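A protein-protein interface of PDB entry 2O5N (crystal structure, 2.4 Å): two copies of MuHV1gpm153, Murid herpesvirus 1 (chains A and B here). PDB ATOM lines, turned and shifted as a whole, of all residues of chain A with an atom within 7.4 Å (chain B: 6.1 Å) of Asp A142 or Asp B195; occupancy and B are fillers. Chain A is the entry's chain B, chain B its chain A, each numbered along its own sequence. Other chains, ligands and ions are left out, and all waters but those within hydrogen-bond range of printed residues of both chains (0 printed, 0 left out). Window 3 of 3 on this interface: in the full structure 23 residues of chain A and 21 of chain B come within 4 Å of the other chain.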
ATOM      1  N   ILE A 129       8.075  -8.094 -21.107  1.00  0.00           N
ATOM      2  CA  ILE A 129       7.990  -8.894 -19.885  1.00  0.00           C
ATOM      3  C   ILE A 129       9.409  -9.381 -19.561  1.00  0.00           C
ATOM      4  O   ILE A 129      10.124  -9.850 -20.442  1.00  0.00           O
ATOM      5  CB  ILE A 129       7.018 -10.104 -20.035  1.00  0.00           C
ATOM      6  CG1 ILE A 129       5.599  -9.631 -20.374  1.00  0.00           C
ATOM      7  CG2 ILE A 129       6.965 -10.943 -18.757  1.00  0.00           C
ATOM      8  CD1 ILE A 129       4.593 -10.759 -20.689  1.00  0.00           C
ATOM      9  N   THR A 133       8.372 -14.629 -13.807  1.00  0.00           N
ATOM     10  CA  THR A 133       6.989 -14.928 -13.443  1.00  0.00           C
ATOM     11  C   THR A 133       6.910 -15.977 -12.340  1.00  0.00           C
ATOM     12  O   THR A 133       6.251 -15.768 -11.318  1.00  0.00           O
ATOM     13  CB  THR A 133       6.192 -15.411 -14.674  1.00  0.00           C
ATOM     14  OG1 THR A 133       6.500 -14.581 -15.803  1.00  0.00           O
ATOM     15  CG2 THR A 133       4.690 -15.365 -14.412  1.00  0.00           C
ATOM     16  N   LYS A 139       0.572 -18.543 -11.932  1.00  0.00           N
ATOM     17  CA  LYS A 139      -0.090 -18.371 -13.217  1.00  0.00           C
ATOM     18  C   LYS A 139       0.907 -18.053 -14.341  1.00  0.00           C
ATOM     19  O   LYS A 139       2.128 -17.988 -14.124  1.00  0.00           O
ATOM     20  CB  LYS A 139      -1.184 -17.303 -13.118  1.00  0.00           C
ATOM     21  N   ASN A 140       0.371 -17.854 -15.538  1.00  0.00           N
ATOM     22  CA  ASN A 140       1.174 -17.788 -16.742  1.00  0.00           C
ATOM     23  C   ASN A 140       1.228 -16.379 -17.354  1.00  0.00           C
ATOM     24  O   ASN A 140       0.441 -15.505 -16.987  1.00  0.00           O
ATOM     25  CB  ASN A 140       0.660 -18.839 -17.739  1.00  0.00           C
ATOM     26  CG  ASN A 140       0.861 -20.268 -17.232  1.00  0.00           C
ATOM     27  OD1 ASN A 140       1.984 -20.676 -16.952  1.00  0.00           O
ATOM     28  ND2 ASN A 140      -0.223 -21.026 -17.116  1.00  0.00           N
ATOM     29  N   GLU A 141       2.170 -16.170 -18.275  1.00  0.00           N
ATOM     30  CA  GLU A 141       2.435 -14.858 -18.874  1.00  0.00           C
ATOM     31  C   GLU A 141       1.221 -14.278 -19.608  1.00  0.00           C
ATOM     32  O   GLU A 141       1.141 -13.068 -19.842  1.00  0.00           O
ATOM     33  CB  GLU A 141       3.650 -14.927 -19.810  1.00  0.00           C
ATOM     34  CG  GLU A 141       5.009 -15.010 -19.107  1.00  0.00           C
ATOM     35  CD  GLU A 141       5.350 -16.411 -18.568  1.00  0.00           C
ATOM     36  OE1 GLU A 141       4.589 -17.372 -18.836  1.00  0.00           O
ATOM     37  OE2 GLU A 141       6.389 -16.550 -17.876  1.00  0.00           O
ATOM     38  N   ASP A 142       0.273 -15.143 -19.955  1.00  0.00           N
ATOM     39  CA  ASP A 142      -0.970 -14.716 -20.596  1.00  0.00           C
ATOM     40  C   ASP A 142      -1.922 -13.998 -19.623  1.00  0.00           C
ATOM     41  O   ASP A 142      -2.743 -13.182 -20.049  1.00  0.00           O
ATOM     42  CB  ASP A 142      -1.661 -15.903 -21.282  1.00  0.00           C
ATOM     43  CG  ASP A 142      -2.471 -16.758 -20.318  1.00  0.00           C
ATOM     44  OD1 ASP A 142      -1.870 -17.427 -19.435  1.00  0.00           O
ATOM     45  OD2 ASP A 142      -3.722 -16.760 -20.466  1.00  0.00           O
ATOM     46  N   THR A 143      -1.811 -14.318 -18.333  1.00  0.00           N
ATOM     47  CA  THR A 143      -2.483 -13.565 -17.271  1.00  0.00           C
ATOM     48  C   THR A 143      -1.870 -12.165 -17.155  1.00  0.00           C
ATOM     49  O   THR A 143      -2.580 -11.176 -17.150  1.00  0.00           O
ATOM     50  CB  THR A 143      -2.382 -14.287 -15.893  1.00  0.00           C
ATOM     51  OG1 THR A 143      -2.835 -15.638 -16.021  1.00  0.00           O
ATOM     52  CG2 THR A 143      -3.214 -13.581 -14.845  1.00  0.00           C
ATOM     53  N   LEU A 144      -0.543 -12.105 -17.063  1.00  0.00           N
ATOM     54  CA  LEU A 144       0.191 -10.843 -16.941  1.00  0.00           C
ATOM     55  C   LEU A 144      -0.218  -9.821 -17.991  1.00  0.00           C
ATOM     56  O   LEU A 144      -0.662  -8.717 -17.661  1.00  0.00           O
ATOM     57  CB  LEU A 144       1.693 -11.092 -17.049  1.00  0.00           C
ATOM     58  CG  LEU A 144       2.361 -12.016 -16.042  1.00  0.00           C
ATOM     59  CD1 LEU A 144       3.847 -12.126 -16.370  1.00  0.00           C
ATOM     60  CD2 LEU A 144       2.148 -11.517 -14.625  1.00  0.00           C
ATOM     61  N   VAL A 145      -0.068 -10.215 -19.252  1.00  0.00           N
ATOM     62  CA  VAL A 145      -0.324  -9.369 -20.419  1.00  0.00           C
ATOM     63  C   VAL A 145      -1.725  -8.709 -20.460  1.00  0.00           C
ATOM     64  O   VAL A 145      -1.955  -7.762 -21.229  1.00  0.00           O
ATOM     65  CB  VAL A 145       0.044 -10.160 -21.731  1.00  0.00           C
ATOM     66  CG1 VAL A 145      -1.120 -10.230 -22.738  1.00  0.00           C
ATOM     67  CG2 VAL A 145       1.303  -9.593 -22.358  1.00  0.00           C
ATOM     68  N   LYS A 146      -2.647  -9.203 -19.630  1.00  0.00           N
ATOM     69  CA  LYS A 146      -3.930  -8.532 -19.412  1.00  0.00           C
ATOM     70  C   LYS A 146      -3.761  -7.182 -18.717  1.00  0.00           C
ATOM     71  O   LYS A 146      -4.651  -6.332 -18.777  1.00  0.00           O
ATOM     72  CB  LYS A 146      -4.844  -9.381 -18.534  1.00  0.00           C
ATOM     73  CG  LYS A 146      -5.668 -10.421 -19.247  1.00  0.00           C
ATOM     74  CD  LYS A 146      -6.797 -10.913 -18.328  1.00  0.00           C
ATOM     75  CE  LYS A 146      -6.283 -11.812 -17.201  1.00  0.00           C
ATOM     76  NZ  LYS A 146      -7.401 -12.356 -16.361  1.00  0.00           N
ATOM     77  N   TYR A 147      -2.629  -7.002 -18.032  1.00  0.00           N
ATOM     78  CA  TYR A 147      -2.423  -5.824 -17.194  1.00  0.00           C
ATOM     79  C   TYR A 147      -1.286  -4.943 -17.641  1.00  0.00           C
ATOM     80  O   TYR A 147      -1.161  -3.833 -17.140  1.00  0.00           O
ATOM     81  CB  TYR A 147      -2.223  -6.228 -15.730  1.00  0.00           C
ATOM     82  CG  TYR A 147      -3.367  -7.045 -15.194  1.00  0.00           C
ATOM     83  CD1 TYR A 147      -4.536  -6.430 -14.738  1.00  0.00           C
ATOM     84  CD2 TYR A 147      -3.297  -8.433 -15.166  1.00  0.00           C
ATOM     85  CE1 TYR A 147      -5.601  -7.179 -14.264  1.00  0.00           C
ATOM     86  CE2 TYR A 147      -4.351  -9.188 -14.698  1.00  0.00           C
ATOM     87  CZ  TYR A 147      -5.493  -8.557 -14.239  1.00  0.00           C
ATOM     88  OH  TYR A 147      -6.531  -9.324 -13.770  1.00  0.00           O
ATOM     89  N   LEU B 192      -0.349 -23.522 -23.556  1.00  0.00           N
ATOM     90  CA  LEU B 192      -1.705 -23.275 -23.081  1.00  0.00           C
ATOM     91  C   LEU B 192      -2.687 -24.160 -23.848  1.00  0.00           C
ATOM     92  O   LEU B 192      -3.314 -23.726 -24.820  1.00  0.00           O
ATOM     93  CB  LEU B 192      -2.078 -21.791 -23.228  1.00  0.00           C
ATOM     94  CG  LEU B 192      -1.288 -20.710 -22.481  1.00  0.00           C
ATOM     95  CD1 LEU B 192      -1.888 -19.353 -22.775  1.00  0.00           C
ATOM     96  CD2 LEU B 192      -1.260 -20.967 -20.984  1.00  0.00           C
ATOM     97  N   GLU B 193      -2.806 -25.407 -23.398  1.00  0.00           N
ATOM     98  CA  GLU B 193      -3.621 -26.430 -24.071  1.00  0.00           C
ATOM     99  C   GLU B 193      -5.131 -26.154 -24.013  1.00  0.00           C
ATOM    100  O   GLU B 193      -5.872 -26.526 -24.927  1.00  0.00           O
ATOM    101  CB  GLU B 193      -3.307 -27.816 -23.489  1.00  0.00           C
ATOM    102  CG  GLU B 193      -1.826 -28.197 -23.561  1.00  0.00           C
ATOM    103  CD  GLU B 193      -1.435 -29.323 -22.605  1.00  0.00           C
ATOM    104  OE1 GLU B 193      -2.263 -29.720 -21.745  1.00  0.00           O
ATOM    105  OE2 GLU B 193      -0.284 -29.807 -22.714  1.00  0.00           O
ATOM    106  N   ASP B 194      -5.571 -25.498 -22.939  1.00  0.00           N
ATOM    107  CA  ASP B 194      -6.992 -25.211 -22.705  1.00  0.00           C
ATOM    108  C   ASP B 194      -7.445 -23.898 -23.337  1.00  0.00           C
ATOM    109  O   ASP B 194      -8.637 -23.684 -23.558  1.00  0.00           O
ATOM    110  CB  ASP B 194      -7.303 -25.203 -21.201  1.00  0.00           C
ATOM    111  CG  ASP B 194      -7.630 -26.597 -20.652  1.00  0.00           C
ATOM    112  OD1 ASP B 194      -7.706 -27.567 -21.447  1.00  0.00           O
ATOM    113  OD2 ASP B 194      -7.819 -26.716 -19.417  1.00  0.00           O
ATOM    114  N   ASP B 195      -6.491 -23.018 -23.615  1.00  0.00           N
ATOM    115  CA  ASP B 195      -6.779 -21.748 -24.266  1.00  0.00           C
ATOM    116  C   ASP B 195      -6.867 -21.967 -25.777  1.00  0.00           C
ATOM    117  O   ASP B 195      -5.910 -22.425 -26.413  1.00  0.00           O
ATOM    118  CB  ASP B 195      -5.697 -20.721 -23.925  1.00  0.00           C
ATOM    119  CG  ASP B 195      -6.209 -19.292 -23.953  1.00  0.00           C
ATOM    120  OD1 ASP B 195      -6.997 -18.940 -24.863  1.00  0.00           O
ATOM    121  OD2 ASP B 195      -5.804 -18.512 -23.061  1.00  0.00           O
ATOM    122  N   ILE B 196      -8.028 -21.651 -26.344  1.00  0.00           N
ATOM    123  CA  ILE B 196      -8.264 -21.847 -27.769  1.00  0.00           C
ATOM    124  C   ILE B 196      -7.658 -20.729 -28.616  1.00  0.00           C
ATOM    125  O   ILE B 196      -7.345 -20.942 -29.791  1.00  0.00           O
ATOM    126  CB  ILE B 196      -9.766 -21.999 -28.052  1.00  0.00           C
ATOM    127  N   GLU B 197      -7.477 -19.549 -28.023  1.00  0.00           N
ATOM    128  CA  GLU B 197      -7.005 -18.374 -28.778  1.00  0.00           C
ATOM    129  C   GLU B 197      -5.597 -17.872 -28.418  1.00  0.00           C
ATOM    130  O   GLU B 197      -4.895 -17.304 -29.268  1.00  0.00           O
ATOM    131  CB  GLU B 197      -8.030 -17.225 -28.726  1.00  0.00           C
ATOM    132  CG  GLU B 197      -8.961 -17.203 -27.505  1.00  0.00           C
ATOM    133  CD  GLU B 197     -10.140 -16.247 -27.684  1.00  0.00           C
ATOM    134  OE1 GLU B 197      -9.921 -15.089 -28.120  1.00  0.00           O
ATOM    135  OE2 GLU B 197     -11.290 -16.650 -27.388  1.00  0.00           O
ATOM    136  N   MET B 198      -5.191 -18.095 -27.170  1.00  0.00           N
ATOM    137  CA  MET B 198      -3.904 -17.612 -26.666  1.00  0.00           C
ATOM    138  C   MET B 198      -2.934 -18.760 -26.387  1.00  0.00           C
ATOM    139  O   MET B 198      -3.339 -19.836 -25.955  1.00  0.00           O
ATOM    140  CB  MET B 198      -4.106 -16.782 -25.388  1.00  0.00           C
ATOM    141  CG  MET B 198      -4.828 -15.448 -25.585  1.00  0.00           C
ATOM    142  SD  MET B 198      -3.763 -14.149 -26.585  1.00  0.00           S
ATOM    143  CE  MET B 198      -2.306 -13.914 -25.294  1.00  0.00           C
ATOM    144  N   ASP B 199      -1.651 -18.524 -26.631  1.00  0.00           N
ATOM    145  CA  ASP B 199      -0.630 -19.522 -26.353  1.00  0.00           C
ATOM    146  C   ASP B 199       0.649 -18.860 -25.847  1.00  0.00           C
ATOM    147  O   ASP B 199       0.831 -17.649 -25.970  1.00  0.00           O
ATOM    148  CB  ASP B 199      -0.349 -20.369 -27.603  1.00  0.00           C
ATOM    149  CG  ASP B 199       0.384 -21.673 -27.293  1.00  0.00           C
ATOM    150  OD1 ASP B 199       0.311 -22.166 -26.150  1.00  0.00           O
ATOM    151  OD2 ASP B 199       1.034 -22.215 -28.210  1.00  0.00           O
ATOM    152  N   ILE B 200       1.522 -19.671 -25.263  1.00  0.00           N
ATOM    153  CA  ILE B 200       2.831 -19.221 -24.831  1.00  0.00           C
ATOM    154  C   ILE B 200       3.909 -19.929 -25.650  1.00  0.00           C
ATOM    155  O   ILE B 200       3.914 -21.162 -25.771  1.00  0.00           O
ATOM    156  CB  ILE B 200       3.021 -19.415 -23.294  1.00  0.00           C
ATOM    157  CG1 ILE B 200       2.132 -18.421 -22.530  1.00  0.00           C
ATOM    158  CG2 ILE B 200       4.488 -19.259 -22.890  1.00  0.00           C
ATOM    159  CD1 ILE B 200       1.874 -18.789 -21.097  1.00  0.00           C
ATOM    160  N   PRO B 244       3.678 -14.661 -24.287  1.00  0.00           N
ATOM    161  CA  PRO B 244       2.271 -14.831 -24.597  1.00  0.00           C
ATOM    162  C   PRO B 244       2.027 -14.314 -26.001  1.00  0.00           C
ATOM    163  O   PRO B 244       2.631 -13.325 -26.416  1.00  0.00           O
ATOM    164  CB  PRO B 244       1.566 -13.957 -23.558  1.00  0.00           C
ATOM    165  CG  PRO B 244       2.543 -12.911 -23.227  1.00  0.00           C
ATOM    166  CD  PRO B 244       3.899 -13.556 -23.333  1.00  0.00           C
ATOM    167  N   ARG B 247      -2.424 -17.232 -31.169  1.00  0.00           N
ATOM    168  CA  ARG B 247      -2.110 -18.425 -31.970  1.00  0.00           C
ATOM    169  C   ARG B 247      -2.087 -18.162 -33.479  1.00  0.00           C
ATOM    170  O   ARG B 247      -1.335 -18.807 -34.211  1.00  0.00           O
ATOM    171  CB  ARG B 247      -3.063 -19.582 -31.644  1.00  0.00           C
ATOM    172  CG  ARG B 247      -2.824 -20.228 -30.285  1.00  0.00           C
ATOM    173  CD  ARG B 247      -3.741 -21.425 -30.065  1.00  0.00           C
ATOM    174  NE  ARG B 247      -3.623 -21.960 -28.712  1.00  0.00           N
ATOM    175  CZ  ARG B 247      -3.005 -23.095 -28.396  1.00  0.00           C
ATOM    176  NH1 ARG B 247      -2.448 -23.850 -29.335  1.00  0.00           N
ATOM    177  NH2 ARG B 247      -2.953 -23.487 -27.133  1.00  0.00           N
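Hydrophobic or aromatic side chains of chain A that line the printed part of chain B: Ile A129 and Val A145. Printed residues of chain B that touch a printed residue of chain A: Leu B192, Asp B195, Ile B200 and Pro B244. Among the printed residues, 8 pairs touch across the chains.
Of the printed residues of chain B, Asn A140 touches Ile B200. Printed residues of chain B within 4 Å of Glu A141: Ile B200 (3.8 Å) and Pro B244 (3.7 Å). Asp A142 touches three residues of chain B. Of the printed residues of chain B, Val A145 touches Pro B244 (3.6 Å). Of the printed residues of chain A, Leu B192 touches Asp A142. Asp B195 touches just one residue of chain A: Asp A142 (3.8 Å). Ile B196 touches none of the printed residues of chain A. Printed residues of chain A within 4 Å of Pro B244: Ile A129 (3.9 Å), Glu A141 (3.7 Å), Asp A142 (3.97 Å) and Val A145 (3.6 Å). The nearest printed residue of chain A that does not touch Asp B195 is Thr A143 (7.5 Å).
No position is printed for both chains. Of the 8 pairs that touch across the chains among the printed residues, none has its exchanged pair printed and touching as well.
Among the printed residues, pairs that only touch across the chains: Asn A140 with Ile B200, Asp A142 with Leu B192, Val A145 with Pro B244, Glu A141 with Pro B244, Asp A142 with Asp B195, Glu A141 with Ile B200, Ile A129 with Pro B244 and Asp A142 with Pro B244.
OD1 of Asp B195 is in hydrogen-bond range of N of Glu B197 (3.3 Å). OD1 of Asp B195 sits at hydrogen-bond distance from N of Met B198, at 3.0 Å. O of Asn A140 sits close to OG1 of Thr A143 (3.4 Å). OG1 of Thr A133 sits at hydrogen-bond distance from OE2 of Glu A141 (2.9 Å). NH2 of Arg B247 is in hydrogen-bond range of O of Asp B195, at 3.2 Å. The backbone NH (N) of Leu B192 lies within hydrogen-bond range of the side-chain carboxylate (OD1) of Asp B199, 3.0 Å away.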
